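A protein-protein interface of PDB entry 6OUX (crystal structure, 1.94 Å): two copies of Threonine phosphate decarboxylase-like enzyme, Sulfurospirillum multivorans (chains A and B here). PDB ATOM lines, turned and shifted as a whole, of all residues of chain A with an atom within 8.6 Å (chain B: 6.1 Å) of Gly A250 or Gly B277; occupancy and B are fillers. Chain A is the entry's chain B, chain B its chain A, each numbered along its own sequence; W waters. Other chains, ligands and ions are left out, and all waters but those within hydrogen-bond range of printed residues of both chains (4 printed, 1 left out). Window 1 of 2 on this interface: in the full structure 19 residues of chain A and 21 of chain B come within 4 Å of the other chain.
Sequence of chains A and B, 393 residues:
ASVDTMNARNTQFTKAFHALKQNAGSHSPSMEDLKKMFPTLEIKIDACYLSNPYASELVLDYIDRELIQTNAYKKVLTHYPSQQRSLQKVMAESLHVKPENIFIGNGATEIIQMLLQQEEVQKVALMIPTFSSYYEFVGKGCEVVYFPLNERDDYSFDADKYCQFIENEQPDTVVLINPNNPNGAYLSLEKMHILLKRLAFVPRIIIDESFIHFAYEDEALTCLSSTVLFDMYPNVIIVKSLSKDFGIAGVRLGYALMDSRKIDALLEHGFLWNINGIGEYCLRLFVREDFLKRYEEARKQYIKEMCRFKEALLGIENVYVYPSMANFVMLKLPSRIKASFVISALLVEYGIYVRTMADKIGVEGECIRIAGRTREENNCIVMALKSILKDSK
Hydrophobic or aromatic side chains of chain A that line the printed part of chain B: Tyr A49 and Ala A249. Among the printed residues, 18 pairs touch across the chains. Among the printed residues, no Asp or Glu carboxylate lies within 4 Å of a Lys or Arg side-chain nitrogen of the other chain.
Gly A250 touches just these residues of chain B: Val B76, Leu B77, His B79, Asn B276 and Gly B277. Of the printed residues of chain A, His B79 touches Tyr A49 (3.8 Å), Ala A249 (3.6 Å) and Gly A250 (3.3 Å). Printed residues of chain A within 4 Å of Pro B81: Ala A249 (3.6 Å). Of chain A, only Gly A250 comes within 4 Å of Gly B277. Tyr B281 touches none of the printed residues of chain A. The nearest residue of chain A that does not touch Gly B277 is Val A251 (5.0 Å).
Among the printed residues, pairs that only touch across the chains: Tyr A49 with His B79 (3.8 Å), Tyr A49 with Tyr B80 (3.2 Å), Leu A50 with Tyr B80 (3.8 Å), Ser A56 with Thr B78 (3.7 Å), Gly A247 with Thr B78 (3.7 Å), Ile A248 with Leu B77 (3.4 Å), Ala A249 with Thr B78 (3.5 Å), Ala A249 with His B79 (3.6 Å), Ala A249 with Tyr B80 (3.2 Å), Ala A249 with Pro B81 (3.6 Å), Gly A250 with Val B76 (3.7 Å), Gly A250 with Asn B276 (3.4 Å) and Arg A252 with Ile B275 (3.8 Å).
The side-chain amide nitrogen of Asn B276 lies close to the side-chain amide nitrogen of Asn A276 (3.0 Å). O of Gly A250 lies within hydrogen-bond range of N of Gly B277. The backbone NH of Gly A250 is in hydrogen-bond range of the backbone carbonyl oxygen of His B79 (3.3 Å). The backbone NH (N) of Gly A250 lies within hydrogen-bond range of the backbone carbonyl oxygen (O) of Leu B77, 2.8 Å away. O of Leu B77 sits at hydrogen-bond distance from N of Ala A249.
Asn A276 touches its own counterpart, Asn B276. Of the 18 pairs that touch across the chains among the printed residues, 1 has its exchanged pair printed and touching as well.
Water W2 lies within hydrogen-bond range of O of Thr B78 (2.6 Å), OG of Ser A51 (2.6 Å), O of Gly A247 (3.1 Å) and N of Ala A249 (3.3 Å). Water W1 lies within hydrogen-bond range of the side-chain hydroxyl of Tyr B80 (2.7 Å) and the backbone NH of Leu A50 (3.2 Å). Water W4 lies within hydrogen-bond range of N of Ile B278 (3.0 Å), O of Gly A250 (3.1 Å) and N of Gly B277 (3.5 Å). Water W3 bridges the guanidinium group of Arg A252 (3.0 Å) and the side-chain amide nitrogen of Asn B276 (3.4 Å).
OD1 of Asn B276 is in hydrogen-bond range of N of Gly B279 (2.9 Å). OG of Ser A56 sits at hydrogen-bond distance from O of Gly A247, 2.5 Å away. OD1 of Asn A276 lies within hydrogen-bond range of N of Gly A279 (2.5 Å). N of Ile A278 is in hydrogen-bond range of OD1 of Asn A276. N of Ile A248 is in hydrogen-bond range of O of Ser A243, 3.4 Å away.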
ATOM      1  N   TYR A  49     -19.642  -3.630 -20.209  1.00  0.00           N
ATOM      2  CA  TYR A  49     -20.437  -2.720 -19.444  1.00  0.00           C
ATOM      3  C   TYR A  49     -19.844  -1.328 -19.364  1.00  0.00           C
ATOM      4  O   TYR A  49     -18.635  -1.176 -19.259  1.00  0.00           O
ATOM      5  CB  TYR A  49     -20.617  -3.282 -17.991  1.00  0.00           C
ATOM      6  CG  TYR A  49     -19.506  -2.990 -16.918  1.00  0.00           C
ATOM      7  CD1 TYR A  49     -18.451  -3.875 -16.723  1.00  0.00           C
ATOM      8  CD2 TYR A  49     -19.573  -1.888 -16.061  1.00  0.00           C
ATOM      9  CE1 TYR A  49     -17.476  -3.641 -15.758  1.00  0.00           C
ATOM     10  CE2 TYR A  49     -18.626  -1.664 -15.075  1.00  0.00           C
ATOM     11  CZ  TYR A  49     -17.572  -2.531 -14.942  1.00  0.00           C
ATOM     12  OH  TYR A  49     -16.635  -2.321 -13.983  1.00  0.00           O
ATOM     13  N   LEU A  50     -20.720  -0.334 -19.267  1.00  0.00           N
ATOM     14  CA  LEU A  50     -20.344   1.095 -19.266  1.00  0.00           C
ATOM     15  C   LEU A  50     -20.177   1.748 -17.869  1.00  0.00           C
ATOM     16  O   LEU A  50     -21.044   1.632 -17.001  1.00  0.00           O
ATOM     17  CB  LEU A  50     -21.373   1.842 -20.063  1.00  0.00           C
ATOM     18  CG  LEU A  50     -21.525   1.236 -21.446  1.00  0.00           C
ATOM     19  CD1 LEU A  50     -22.609   1.969 -22.157  1.00  0.00           C
ATOM     20  CD2 LEU A  50     -20.186   1.262 -22.247  1.00  0.00           C
ATOM     21  N   SER A  51     -19.075   2.453 -17.654  1.00  0.00           N
ATOM     22  CA  SER A  51     -18.920   3.157 -16.393  1.00  0.00           C
ATOM     23  C   SER A  51     -17.947   4.359 -16.473  1.00  0.00           C
ATOM     24  O   SER A  51     -17.547   4.781 -17.548  1.00  0.00           O
ATOM     25  CB  SER A  51     -18.494   2.120 -15.326  1.00  0.00           C
ATOM     26  OG  SER A  51     -18.585   2.592 -13.959  1.00  0.00           O
ATOM     27  N   SER A  56     -16.810   6.203  -9.972  1.00  0.00           N
ATOM     28  CA  SER A  56     -16.951   5.118  -8.965  1.00  0.00           C
ATOM     29  C   SER A  56     -16.105   5.332  -7.731  1.00  0.00           C
ATOM     30  O   SER A  56     -16.619   5.270  -6.658  1.00  0.00           O
ATOM     31  CB  SER A  56     -16.494   3.774  -9.499  1.00  0.00           C
ATOM     32  OG  SER A  56     -17.423   3.341 -10.389  1.00  0.00           O
ATOM     33  N   SER A 243     -26.543   5.947 -13.464  1.00  0.00           N
ATOM     34  CA  SER A 243     -25.525   4.903 -13.199  1.00  0.00           C
ATOM     35  C   SER A 243     -24.330   4.802 -14.147  1.00  0.00           C
ATOM     36  O   SER A 243     -23.300   4.360 -13.721  1.00  0.00           O
ATOM     37  CB  SER A 243     -26.123   3.554 -13.108  1.00  0.00           C
ATOM     38  OG  SER A 243     -26.988   3.315 -14.141  1.00  0.00           O
ATOM     39  N   GLY A 247     -20.965   5.760 -12.142  1.00  0.00           N
ATOM     40  CA  GLY A 247     -20.179   4.522 -11.894  1.00  0.00           C
ATOM     41  C   GLY A 247     -20.695   3.607 -10.786  1.00  0.00           C
ATOM     42  O   GLY A 247     -19.900   3.034 -10.003  1.00  0.00           O
ATOM     43  N   ILE A 248     -22.024   3.521 -10.687  1.00  0.00           N
ATOM     44  CA  ILE A 248     -22.695   2.717  -9.696  1.00  0.00           C
ATOM     45  C   ILE A 248     -23.584   1.689 -10.386  1.00  0.00           C
ATOM     46  O   ILE A 248     -24.827   1.676 -10.208  1.00  0.00           O
ATOM     47  CB  ILE A 248     -23.504   3.592  -8.720  1.00  0.00           C
ATOM     48  CG1 ILE A 248     -24.398   4.583  -9.513  1.00  0.00           C
ATOM     49  CG2 ILE A 248     -22.556   4.445  -7.885  1.00  0.00           C
ATOM     50  CD1 ILE A 248     -25.595   5.100  -8.745  1.00  0.00           C
ATOM     51  N   ALA A 249     -22.966   0.788 -11.136  1.00  0.00           N
ATOM     52  CA  ALA A 249     -23.783  -0.228 -11.901  1.00  0.00           C
ATOM     53  C   ALA A 249     -24.589  -1.151 -11.009  1.00  0.00           C
ATOM     54  O   ALA A 249     -25.618  -1.643 -11.426  1.00  0.00           O
ATOM     55  CB  ALA A 249     -22.930  -1.010 -12.859  1.00  0.00           C
ATOM     56  N   GLY A 250     -24.221  -1.311  -9.746  1.00  0.00           N
ATOM     57  CA  GLY A 250     -25.054  -2.102  -8.833  1.00  0.00           C
ATOM     58  C   GLY A 250     -26.260  -1.454  -8.202  1.00  0.00           C
ATOM     59  O   GLY A 250     -26.918  -2.036  -7.333  1.00  0.00           O
ATOM     60  N   VAL A 251     -26.521  -0.201  -8.584  1.00  0.00           N
ATOM     61  CA  VAL A 251     -27.609   0.541  -8.035  1.00  0.00           C
ATOM     62  C   VAL A 251     -28.408   0.907  -9.276  1.00  0.00           C
ATOM     63  O   VAL A 251     -27.833   1.253 -10.298  1.00  0.00           O
ATOM     64  CB  VAL A 251     -27.049   1.809  -7.348  1.00  0.00           C
ATOM     65  CG1 VAL A 251     -28.151   2.655  -6.733  1.00  0.00           C
ATOM     66  CG2 VAL A 251     -25.989   1.426  -6.340  1.00  0.00           C
ATOM     67  N   ARG A 252     -29.712   0.798  -9.258  1.00  0.00           N
ATOM     68  CA  ARG A 252     -30.393   1.109 -10.492  1.00  0.00           C
ATOM     69  C   ARG A 252     -31.014   2.465 -10.357  1.00  0.00           C
ATOM     70  O   ARG A 252     -31.895   2.599  -9.567  1.00  0.00           O
ATOM     71  CB  ARG A 252     -31.481   0.067 -10.769  1.00  0.00           C
ATOM     72  CG  ARG A 252     -30.900  -1.294 -11.135  1.00  0.00           C
ATOM     73  CD  ARG A 252     -31.955  -2.369 -10.861  1.00  0.00           C
ATOM     74  NE  ARG A 252     -33.117  -2.306 -11.775  1.00  0.00           N
ATOM     75  CZ  ARG A 252     -34.406  -2.321 -11.407  1.00  0.00           C
ATOM     76  NH1 ARG A 252     -34.773  -2.374 -10.118  1.00  0.00           N
ATOM     77  NH2 ARG A 252     -35.352  -2.279 -12.345  1.00  0.00           N
ATOM     78  N   LEU A 253     -30.601   3.443 -11.170  1.00  0.00           N
ATOM     79  CA  LEU A 253     -31.144   4.771 -11.041  1.00  0.00           C
ATOM     80  C   LEU A 253     -31.163   5.606 -12.290  1.00  0.00           C
ATOM     81  O   LEU A 253     -30.183   5.657 -13.024  1.00  0.00           O
ATOM     82  CB  LEU A 253     -30.322   5.502  -9.976  1.00  0.00           C
ATOM     83  CG  LEU A 253     -30.945   6.474  -9.037  1.00  0.00           C
ATOM     84  CD1 LEU A 253     -32.193   5.938  -8.334  1.00  0.00           C
ATOM     85  CD2 LEU A 253     -29.833   6.871  -8.033  1.00  0.00           C
ATOM     86  N   ASN A 276     -34.666   2.036  -3.249  1.00  0.00           N
ATOM     87  CA  ASN A 276     -34.190   1.704  -1.900  1.00  0.00           C
ATOM     88  C   ASN A 276     -33.409   2.863  -1.283  1.00  0.00           C
ATOM     89  O   ASN A 276     -33.219   3.908  -1.927  1.00  0.00           O
ATOM     90  CB  ASN A 276     -33.322   0.442  -1.929  1.00  0.00           C
ATOM     91  CG  ASN A 276     -32.044   0.613  -2.739  1.00  0.00           C
ATOM     92  OD1 ASN A 276     -31.583   1.722  -2.968  1.00  0.00           O
ATOM     93  ND2 ASN A 276     -31.459  -0.498  -3.159  1.00  0.00           N
ATOM     94  N   ILE A 278     -30.179   2.882  -0.636  1.00  0.00           N
ATOM     95  CA  ILE A 278     -28.865   3.090  -1.318  1.00  0.00           C
ATOM     96  C   ILE A 278     -29.029   4.019  -2.507  1.00  0.00           C
ATOM     97  O   ILE A 278     -28.281   4.971  -2.676  1.00  0.00           O
ATOM     98  CB  ILE A 278     -28.239   1.777  -1.810  1.00  0.00           C
ATOM     99  CG1 ILE A 278     -28.040   0.792  -0.642  1.00  0.00           C
ATOM    100  CG2 ILE A 278     -26.903   2.047  -2.462  1.00  0.00           C
ATOM    101  CD1 ILE A 278     -27.348   1.381   0.566  1.00  0.00           C
ATOM    102  N   GLY A 279     -30.034   3.706  -3.322  1.00  0.00           N
ATOM    103  CA  GLY A 279     -30.453   4.526  -4.420  1.00  0.00           C
ATOM    104  C   GLY A 279     -30.764   5.945  -4.020  1.00  0.00           C
ATOM    105  O   GLY A 279     -30.304   6.894  -4.675  1.00  0.00           O
ATOM    106  N   CYS A 282     -27.735   7.911  -2.968  1.00  0.00           N
ATOM    107  CA  CYS A 282     -26.983   8.293  -4.158  1.00  0.00           C
ATOM    108  C   CYS A 282     -27.654   9.430  -4.855  1.00  0.00           C
ATOM    109  O   CYS A 282     -26.993  10.364  -5.265  1.00  0.00           O
ATOM    110  CB  CYS A 282     -26.771   7.112  -5.149  1.00  0.00           C
ATOM    111  SG  CYS A 282     -25.601   5.871  -4.599  1.00  0.00           S
ATOM    112  N   VAL B  76     -19.875  -4.858  -4.986  1.00  0.00           N
ATOM    113  CA  VAL B  76     -21.343  -5.048  -5.038  1.00  0.00           C
ATOM    114  C   VAL B  76     -22.036  -3.785  -5.621  1.00  0.00           C
ATOM    115  O   VAL B  76     -22.982  -3.884  -6.404  1.00  0.00           O
ATOM    116  CB  VAL B  76     -21.947  -5.396  -3.635  1.00  0.00           C
ATOM    117  CG1 VAL B  76     -23.487  -5.345  -3.648  1.00  0.00           C
ATOM    118  CG2 VAL B  76     -21.453  -6.743  -3.131  1.00  0.00           C
ATOM    119  N   LEU B  77     -21.537  -2.601  -5.284  1.00  0.00           N
ATOM    120  CA  LEU B  77     -22.170  -1.342  -5.735  1.00  0.00           C
ATOM    121  C   LEU B  77     -21.735  -0.901  -7.133  1.00  0.00           C
ATOM    122  O   LEU B  77     -22.476  -0.229  -7.826  1.00  0.00           O
ATOM    123  CB  LEU B  77     -21.897  -0.256  -4.705  1.00  0.00           C
ATOM    124  CG  LEU B  77     -22.546  -0.493  -3.291  1.00  0.00           C
ATOM    125  CD1 LEU B  77     -22.184   0.617  -2.306  1.00  0.00           C
ATOM    126  CD2 LEU B  77     -24.060  -0.667  -3.362  1.00  0.00           C
ATOM    127  N   THR B  78     -20.558  -1.353  -7.532  1.00  0.00           N
ATOM    128  CA  THR B  78     -19.824  -0.876  -8.683  1.00  0.00           C
ATOM    129  C   THR B  78     -19.988  -1.739  -9.939  1.00  0.00           C
ATOM    130  O   THR B  78     -19.996  -1.211 -11.043  1.00  0.00           O
ATOM    131  CB  THR B  78     -18.322  -0.731  -8.204  1.00  0.00           C
ATOM    132  OG1 THR B  78     -18.037   0.652  -7.956  1.00  0.00           O
ATOM    133  CG2 THR B  78     -17.317  -1.427  -9.035  1.00  0.00           C
ATOM    134  N   HIS B  79     -20.123  -3.048  -9.781  1.00  0.00           N
ATOM    135  CA  HIS B  79     -20.202  -3.981 -10.913  1.00  0.00           C
ATOM    136  C   HIS B  79     -21.622  -4.191 -11.393  1.00  0.00           C
ATOM    137  O   HIS B  79     -22.550  -4.049 -10.605  1.00  0.00           O
ATOM    138  CB  HIS B  79     -19.578  -5.315 -10.511  1.00  0.00           C
ATOM    139  CG  HIS B  79     -18.081  -5.279 -10.452  1.00  0.00           C
ATOM    140  ND1 HIS B  79     -17.326  -6.345 -10.015  1.00  0.00           N
ATOM    141  CD2 HIS B  79     -17.201  -4.293 -10.749  1.00  0.00           C
ATOM    142  CE1 HIS B  79     -16.046  -6.028 -10.072  1.00  0.00           C
ATOM    143  NE2 HIS B  79     -15.944  -4.784 -10.507  1.00  0.00           N
ATOM    144  N   TYR B  80     -21.795  -4.496 -12.683  1.00  0.00           N
ATOM    145  CA  TYR B  80     -23.123  -4.841 -13.209  1.00  0.00           C
ATOM    146  C   TYR B  80     -23.589  -6.155 -12.572  1.00  0.00           C
ATOM    147  O   TYR B  80     -22.805  -7.096 -12.471  1.00  0.00           O
ATOM    148  CB  TYR B  80     -23.164  -5.018 -14.744  1.00  0.00           C
ATOM    149  CG  TYR B  80     -23.532  -3.762 -15.444  1.00  0.00           C
ATOM    150  CD1 TYR B  80     -24.798  -3.551 -15.955  1.00  0.00           C
ATOM    151  CD2 TYR B  80     -22.619  -2.730 -15.524  1.00  0.00           C
ATOM    152  CE1 TYR B  80     -25.114  -2.358 -16.579  1.00  0.00           C
ATOM    153  CE2 TYR B  80     -22.930  -1.534 -16.144  1.00  0.00           C
ATOM    154  CZ  TYR B  80     -24.169  -1.355 -16.668  1.00  0.00           C
ATOM    155  OH  TYR B  80     -24.412  -0.145 -17.272  1.00  0.00           O
ATOM    156  N   PRO B  81     -24.852  -6.204 -12.139  1.00  0.00           N
ATOM    157  CA  PRO B  81     -25.285  -7.408 -11.458  1.00  0.00           C
ATOM    158  C   PRO B  81     -25.696  -8.471 -12.471  1.00  0.00           C
ATOM    159  O   PRO B  81     -25.987  -8.164 -13.621  1.00  0.00           O
ATOM    160  CB  PRO B  81     -26.503  -6.959 -10.681  1.00  0.00           C
ATOM    161  CG  PRO B  81     -26.587  -5.490 -10.839  1.00  0.00           C
ATOM    162  CD  PRO B  81     -25.883  -5.171 -12.103  1.00  0.00           C
ATOM    163  N   ILE B 275     -32.061  -7.035 -10.929  1.00  0.00           N
ATOM    164  CA  ILE B 275     -31.775  -7.051  -9.499  1.00  0.00           C
ATOM    165  C   ILE B 275     -30.699  -5.991  -9.221  1.00  0.00           C
ATOM    166  O   ILE B 275     -30.032  -5.531 -10.126  1.00  0.00           O
ATOM    167  CB  ILE B 275     -31.320  -8.450  -9.057  1.00  0.00           C
ATOM    168  CG1 ILE B 275     -31.480  -8.616  -7.549  1.00  0.00           C
ATOM    169  CG2 ILE B 275     -29.879  -8.737  -9.505  1.00  0.00           C
ATOM    170  CD1 ILE B 275     -31.332 -10.070  -7.141  1.00  0.00           C
ATOM    171  N   ASN B 276     -30.537  -5.568  -7.980  1.00  0.00           N
ATOM    172  CA  ASN B 276     -29.459  -4.625  -7.677  1.00  0.00           C
ATOM    173  C   ASN B 276     -28.351  -5.431  -7.040  1.00  0.00           C
ATOM    174  O   ASN B 276     -28.568  -6.602  -6.718  1.00  0.00           O
ATOM    175  CB  ASN B 276     -29.921  -3.452  -6.796  1.00  0.00           C
ATOM    176  CG  ASN B 276     -30.743  -3.874  -5.573  1.00  0.00           C
ATOM    177  OD1 ASN B 276     -30.709  -4.996  -5.159  1.00  0.00           O
ATOM    178  ND2 ASN B 276     -31.502  -2.926  -4.986  1.00  0.00           N
ATOM    179  N   GLY B 277     -27.201  -4.809  -6.803  1.00  0.00           N
ATOM    180  CA  GLY B 277     -26.054  -5.519  -6.214  1.00  0.00           C
ATOM    181  C   GLY B 277     -26.402  -6.187  -4.896  1.00  0.00           C
ATOM    182  O   GLY B 277     -26.060  -7.351  -4.647  1.00  0.00           O
ATOM    183  N   ILE B 278     -26.968  -5.418  -3.986  1.00  0.00           N
ATOM    184  CA  ILE B 278     -27.190  -5.922  -2.617  1.00  0.00           C
ATOM    185  C   ILE B 278     -28.232  -7.026  -2.661  1.00  0.00           C
ATOM    186  O   ILE B 278     -28.098  -7.973  -1.927  1.00  0.00           O
ATOM    187  CB  ILE B 278     -27.543  -4.807  -1.594  1.00  0.00           C
ATOM    188  CG1 ILE B 278     -27.606  -5.314  -0.141  1.00  0.00           C
ATOM    189  CG2 ILE B 278     -28.864  -4.146  -1.914  1.00  0.00           C
ATOM    190  CD1 ILE B 278     -26.291  -5.945   0.300  1.00  0.00           C
ATOM    191  N   GLY B 279     -29.231  -6.897  -3.544  1.00  0.00           N
ATOM    192  CA  GLY B 279     -30.239  -7.906  -3.779  1.00  0.00           C
ATOM    193  C   GLY B 279     -29.638  -9.237  -4.177  1.00  0.00           C
ATOM    194  O   GLY B 279     -30.014 -10.298  -3.613  1.00  0.00           O
ATOM    195  N   GLU B 280     -28.744  -9.183  -5.164  1.00  0.00           N
ATOM    196  CA  GLU B 280     -28.023 -10.353  -5.614  1.00  0.00           C
ATOM    197  C   GLU B 280     -27.203 -11.017  -4.539  1.00  0.00           C
ATOM    198  O   GLU B 280     -27.259 -12.224  -4.446  1.00  0.00           O
ATOM    199  CB  GLU B 280     -27.112 -10.038  -6.782  1.00  0.00           C
ATOM    200  CG  GLU B 280     -26.401 -11.257  -7.278  1.00  0.00           C
ATOM    201  CD  GLU B 280     -25.589 -10.997  -8.535  1.00  0.00           C
ATOM    202  OE1 GLU B 280     -25.613  -9.874  -9.103  1.00  0.00           O
ATOM    203  OE2 GLU B 280     -24.891 -11.936  -8.922  1.00  0.00           O
ATOM    204  N   TYR B 281     -26.414 -10.242  -3.779  1.00  0.00           N
ATOM    205  CA  TYR B 281     -25.650 -10.760  -2.659  1.00  0.00           C
ATOM    206  C   TYR B 281     -26.612 -11.571  -1.752  1.00  0.00           C
ATOM    207  O   TYR B 281     -26.317 -12.692  -1.342  1.00  0.00           O
ATOM    208  CB  TYR B 281     -25.029  -9.630  -1.824  1.00  0.00           C
ATOM    209  CG  TYR B 281     -24.469 -10.147  -0.527  1.00  0.00           C
ATOM    210  CD1 TYR B 281     -23.203 -10.772  -0.495  1.00  0.00           C
ATOM    211  CD2 TYR B 281     -25.213 -10.131   0.645  1.00  0.00           C
ATOM    212  CE1 TYR B 281     -22.679 -11.311   0.689  1.00  0.00           C
ATOM    213  CE2 TYR B 281     -24.696 -10.708   1.826  1.00  0.00           C
ATOM    214  CZ  TYR B 281     -23.443 -11.296   1.838  1.00  0.00           C
ATOM    215  OH  TYR B 281     -22.914 -11.845   3.000  1.00  0.00           O
ATOM    216  N   CYS B 282     -27.751 -10.984  -1.451  1.00  0.00           N
ATOM    217  CA  CYS B 282     -28.677 -11.600  -0.492  1.00  0.00           C
ATOM    218  C   CYS B 282     -29.275 -12.863  -1.066  1.00  0.00           C
ATOM    219  O   CYS B 282     -29.412 -13.869  -0.379  1.00  0.00           O
ATOM    220  CB  CYS B 282     -29.799 -10.631  -0.124  1.00  0.00           C
ATOM    221  SG  CYS B 282     -29.314  -9.333   1.035  1.00  0.00           S
HETATM  222  O   HOH W   1     -23.822  -1.168 -19.752  1.00  0.00           O
HETATM  223  O   HOH W   2     -19.896   1.009 -12.353  1.00  0.00           O
HETATM  224  O   HOH W   3     -33.204  -1.626  -7.613  1.00  0.00           O
HETATM  225  O   HOH W   4     -27.236  -2.457  -4.241  1.00  0.00           O
